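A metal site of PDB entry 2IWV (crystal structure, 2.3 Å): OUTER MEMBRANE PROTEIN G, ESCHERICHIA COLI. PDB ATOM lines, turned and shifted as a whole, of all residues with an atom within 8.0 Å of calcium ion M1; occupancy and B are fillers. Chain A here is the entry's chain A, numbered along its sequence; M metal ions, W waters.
The side-chain hydroxyl (OH) of Tyr 23 lies within hydrogen-bond range of the side-chain sulfur (SD) of Met 27. The side-chain amide oxygen (OD1) of Asn 19 sits close to the backbone NH (N) of Gly 29 (2.9 Å). O of Asp 28 lies close to OD1 of Asn 19 (3.1 Å). The backbone NH of Val 56 sits at hydrogen-bond distance from the backbone carbonyl oxygen of Gly 29 (3.0 Å).
Merely in contact with calcium ion M1: Gly 29.
Calcium ion M1 is bound by water W2 (1.8 Å), the side-chain carboxylate of Asp 26 (2.3 Å), the backbone carbonyl oxygen of Met 27 (2.3 Å), the backbone carbonyl oxygen of Gly 22 (2.4 Å), the backbone carbonyl oxygen of Val 20 (2.4 Å), the side-chain amide oxygen of Asn 19 (2.5 Å) and water W1 (2.6 Å). Calcium ion M1 has seven donor atoms within binding distance.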
ATOM      1  N   GLU A  18      -5.237 -10.570  -7.879  1.00  0.00           N
ATOM      2  CA  GLU A  18      -4.930  -9.128  -7.802  1.00  0.00           C
ATOM      3  C   GLU A  18      -3.442  -8.913  -7.898  1.00  0.00           C
ATOM      4  O   GLU A  18      -2.678  -9.584  -7.215  1.00  0.00           O
ATOM      5  CB  GLU A  18      -5.394  -8.538  -6.488  1.00  0.00           C
ATOM      6  CG  GLU A  18      -6.885  -8.590  -6.320  1.00  0.00           C
ATOM      7  CD  GLU A  18      -7.313  -8.181  -4.895  1.00  0.00           C
ATOM      8  OE1 GLU A  18      -6.970  -8.917  -3.905  1.00  0.00           O
ATOM      9  OE2 GLU A  18      -7.988  -7.108  -4.789  1.00  0.00           O
ATOM     10  N   ASN A  19      -3.027  -7.978  -8.751  1.00  0.00           N
ATOM     11  CA  ASN A  19      -1.600  -7.854  -9.020  1.00  0.00           C
ATOM     12  C   ASN A  19      -1.260  -6.459  -9.523  1.00  0.00           C
ATOM     13  O   ASN A  19      -1.891  -6.025 -10.480  1.00  0.00           O
ATOM     14  CB  ASN A  19      -1.168  -8.953 -10.052  1.00  0.00           C
ATOM     15  CG  ASN A  19       0.247  -8.786 -10.578  1.00  0.00           C
ATOM     16  OD1 ASN A  19       1.257  -8.962  -9.865  1.00  0.00           O
ATOM     17  ND2 ASN A  19       0.342  -8.409 -11.835  1.00  0.00           N
ATOM     18  N   VAL A  20      -0.321  -5.793  -8.833  1.00  0.00           N
ATOM     19  CA  VAL A  20       0.310  -4.542  -9.241  1.00  0.00           C
ATOM     20  C   VAL A  20       1.473  -4.925 -10.126  1.00  0.00           C
ATOM     21  O   VAL A  20       2.339  -5.704  -9.706  1.00  0.00           O
ATOM     22  CB  VAL A  20       0.906  -3.810  -8.032  1.00  0.00           C
ATOM     23  CG1 VAL A  20       1.497  -2.489  -8.420  1.00  0.00           C
ATOM     24  CG2 VAL A  20      -0.176  -3.576  -6.967  1.00  0.00           C
ATOM     25  N   GLU A  21       1.519  -4.404 -11.375  1.00  0.00           N
ATOM     26  CA  GLU A  21       2.525  -4.953 -12.232  1.00  0.00           C
ATOM     27  C   GLU A  21       3.905  -4.482 -11.868  1.00  0.00           C
ATOM     28  O   GLU A  21       4.077  -3.419 -11.244  1.00  0.00           O
ATOM     29  CB  GLU A  21       2.177  -4.900 -13.696  1.00  0.00           C
ATOM     30  CG  GLU A  21       1.466  -3.638 -14.129  1.00  0.00           C
ATOM     31  CD  GLU A  21       1.419  -3.535 -15.628  1.00  0.00           C
ATOM     32  OE1 GLU A  21       2.490  -3.329 -16.253  1.00  0.00           O
ATOM     33  OE2 GLU A  21       0.315  -3.669 -16.204  1.00  0.00           O
ATOM     34  N   GLY A  22       4.881  -5.331 -12.146  1.00  0.00           N
ATOM     35  CA  GLY A  22       6.175  -5.265 -11.490  1.00  0.00           C
ATOM     36  C   GLY A  22       6.235  -6.380 -10.467  1.00  0.00           C
ATOM     37  O   GLY A  22       5.198  -6.932 -10.060  1.00  0.00           O
ATOM     38  N   TYR A  23       7.450  -6.716 -10.062  1.00  0.00           N
ATOM     39  CA  TYR A  23       7.688  -7.724  -9.030  1.00  0.00           C
ATOM     40  C   TYR A  23       7.923  -7.005  -7.713  1.00  0.00           C
ATOM     41  O   TYR A  23       9.046  -6.905  -7.197  1.00  0.00           O
ATOM     42  CB  TYR A  23       8.897  -8.587  -9.399  1.00  0.00           C
ATOM     43  CG  TYR A  23       9.017  -9.872  -8.633  1.00  0.00           C
ATOM     44  CD1 TYR A  23       8.340 -11.018  -9.047  1.00  0.00           C
ATOM     45  CD2 TYR A  23       9.810  -9.948  -7.496  1.00  0.00           C
ATOM     46  CE1 TYR A  23       8.463 -12.196  -8.351  1.00  0.00           C
ATOM     47  CE2 TYR A  23       9.934 -11.120  -6.779  1.00  0.00           C
ATOM     48  CZ  TYR A  23       9.255 -12.237  -7.206  1.00  0.00           C
ATOM     49  OH  TYR A  23       9.374 -13.398  -6.460  1.00  0.00           O
ATOM     50  N   GLY A  24       6.819  -6.453  -7.212  1.00  0.00           N
ATOM     51  CA  GLY A  24       6.773  -5.653  -6.016  1.00  0.00           C
ATOM     52  C   GLY A  24       6.493  -6.576  -4.868  1.00  0.00           C
ATOM     53  O   GLY A  24       6.923  -7.739  -4.879  1.00  0.00           O
ATOM     54  N   GLU A  25       5.761  -6.062  -3.889  1.00  0.00           N
ATOM     55  CA  GLU A  25       5.470  -6.849  -2.698  1.00  0.00           C
ATOM     56  C   GLU A  25       4.503  -8.011  -2.989  1.00  0.00           C
ATOM     57  O   GLU A  25       4.551  -9.007  -2.292  1.00  0.00           O
ATOM     58  CB  GLU A  25       4.998  -5.901  -1.559  1.00  0.00           C
ATOM     59  CG  GLU A  25       4.021  -6.494  -0.569  1.00  0.00           C
ATOM     60  CD  GLU A  25       4.336  -6.118   0.858  1.00  0.00           C
ATOM     61  OE1 GLU A  25       4.658  -7.038   1.651  1.00  0.00           O
ATOM     62  OE2 GLU A  25       4.267  -4.917   1.197  1.00  0.00           O
ATOM     63  N   ASP A  26       3.672  -7.895  -4.030  1.00  0.00           N
ATOM     64  CA  ASP A  26       2.652  -8.921  -4.348  1.00  0.00           C
ATOM     65  C   ASP A  26       3.080  -9.928  -5.399  1.00  0.00           C
ATOM     66  O   ASP A  26       2.342 -10.227  -6.304  1.00  0.00           O
ATOM     67  CB  ASP A  26       1.293  -8.276  -4.711  1.00  0.00           C
ATOM     68  CG  ASP A  26       1.224  -7.675  -6.152  1.00  0.00           C
ATOM     69  OD1 ASP A  26       0.207  -6.973  -6.460  1.00  0.00           O
ATOM     70  OD2 ASP A  26       2.135  -7.868  -6.986  1.00  0.00           O
ATOM     71  N   MET A  27       4.230 -10.494  -5.203  1.00  0.00           N
ATOM     72  CA  MET A  27       5.204 -10.724  -6.279  1.00  0.00           C
ATOM     73  C   MET A  27       4.691 -10.719  -7.722  1.00  0.00           C
ATOM     74  O   MET A  27       4.604  -9.649  -8.316  1.00  0.00           O
ATOM     75  CB  MET A  27       6.012 -11.959  -5.952  1.00  0.00           C
ATOM     76  CG  MET A  27       6.453 -11.960  -4.523  1.00  0.00           C
ATOM     77  SD  MET A  27       7.097 -13.517  -4.018  1.00  0.00           S
ATOM     78  CE  MET A  27       5.827 -14.373  -3.185  1.00  0.00           C
ATOM     79  N   ASP A  28       4.347 -11.895  -8.264  1.00  0.00           N
ATOM     80  CA  ASP A  28       3.644 -12.080  -9.542  1.00  0.00           C
ATOM     81  C   ASP A  28       2.157 -11.819  -9.474  1.00  0.00           C
ATOM     82  O   ASP A  28       1.447 -11.969 -10.467  1.00  0.00           O
ATOM     83  CB  ASP A  28       3.834 -13.507 -10.093  1.00  0.00           C
ATOM     84  CG  ASP A  28       5.235 -13.764 -10.644  1.00  0.00           C
ATOM     85  OD1 ASP A  28       5.651 -14.938 -10.633  1.00  0.00           O
ATOM     86  OD2 ASP A  28       5.917 -12.808 -11.089  1.00  0.00           O
ATOM     87  N   GLY A  29       1.676 -11.397  -8.301  1.00  0.00           N
ATOM     88  CA  GLY A  29       0.256 -11.144  -8.025  1.00  0.00           C
ATOM     89  C   GLY A  29      -0.209 -11.892  -6.784  1.00  0.00           C
ATOM     90  O   GLY A  29       0.449 -12.854  -6.330  1.00  0.00           O
ATOM     91  N   LEU A  30      -1.325 -11.431  -6.237  1.00  0.00           N
ATOM     92  CA  LEU A  30      -2.022 -12.046  -5.115  1.00  0.00           C
ATOM     93  C   LEU A  30      -3.047 -12.992  -5.738  1.00  0.00           C
ATOM     94  O   LEU A  30      -3.835 -12.530  -6.595  1.00  0.00           O
ATOM     95  CB  LEU A  30      -2.795 -10.965  -4.361  1.00  0.00           C
ATOM     96  CG  LEU A  30      -2.401 -10.432  -2.988  1.00  0.00           C
ATOM     97  CD1 LEU A  30      -0.963 -10.191  -2.867  1.00  0.00           C
ATOM     98  CD2 LEU A  30      -3.169  -9.103  -2.693  1.00  0.00           C
ATOM     99  N   PRO A  55       0.799 -13.516  -1.893  1.00  0.00           N
ATOM    100  CA  PRO A  55       1.540 -13.379  -3.131  1.00  0.00           C
ATOM    101  C   PRO A  55       2.164 -14.692  -3.678  1.00  0.00           C
ATOM    102  O   PRO A  55       2.401 -15.683  -2.908  1.00  0.00           O
ATOM    103  CB  PRO A  55       2.608 -12.322  -2.813  1.00  0.00           C
ATOM    104  CG  PRO A  55       2.794 -12.391  -1.330  1.00  0.00           C
ATOM    105  CD  PRO A  55       1.489 -12.854  -0.761  1.00  0.00           C
ATOM    106  N   VAL A  56       2.395 -14.703  -4.994  1.00  0.00           N
ATOM    107  CA  VAL A  56       2.937 -15.892  -5.662  1.00  0.00           C
ATOM    108  C   VAL A  56       4.122 -15.595  -6.558  1.00  0.00           C
ATOM    109  O   VAL A  56       4.158 -14.578  -7.257  1.00  0.00           O
ATOM    110  CB  VAL A  56       1.859 -16.733  -6.480  1.00  0.00           C
ATOM    111  CG1 VAL A  56       2.466 -18.067  -7.002  1.00  0.00           C
ATOM    112  CG2 VAL A  56       0.626 -17.071  -5.651  1.00  0.00           C
ATOM    113  N   LYS A 269       0.046   0.263 -11.947  1.00  0.00           N
ATOM    114  CA  LYS A 269      -1.042  -0.278 -12.782  1.00  0.00           C
ATOM    115  C   LYS A 269      -1.452  -1.580 -12.139  1.00  0.00           C
ATOM    116  O   LYS A 269      -0.633  -2.419 -11.849  1.00  0.00           O
ATOM    117  CB  LYS A 269      -0.608  -0.558 -14.237  1.00  0.00           C
ATOM    118  CG  LYS A 269       0.355   0.447 -14.847  1.00  0.00           C
ATOM    119  CD  LYS A 269      -0.321   1.408 -15.844  1.00  0.00           C
ATOM    120  CE  LYS A 269      -0.352   0.805 -17.240  1.00  0.00           C
ATOM    121  NZ  LYS A 269       0.933   0.078 -17.557  1.00  0.00           N
HETATM  122 CA    CA M   1       3.264  -7.848  -8.976  1.00  0.00          CA
HETATM  123 CA    CA M   2       4.743  -3.841  -8.603  1.00  0.00          CA
HETATM  124  O   HOH W   1       4.132  -6.179  -7.217  1.00  0.00           O
HETATM  125  O   HOH W   2       3.714  -8.835 -10.472  1.00  0.00           O
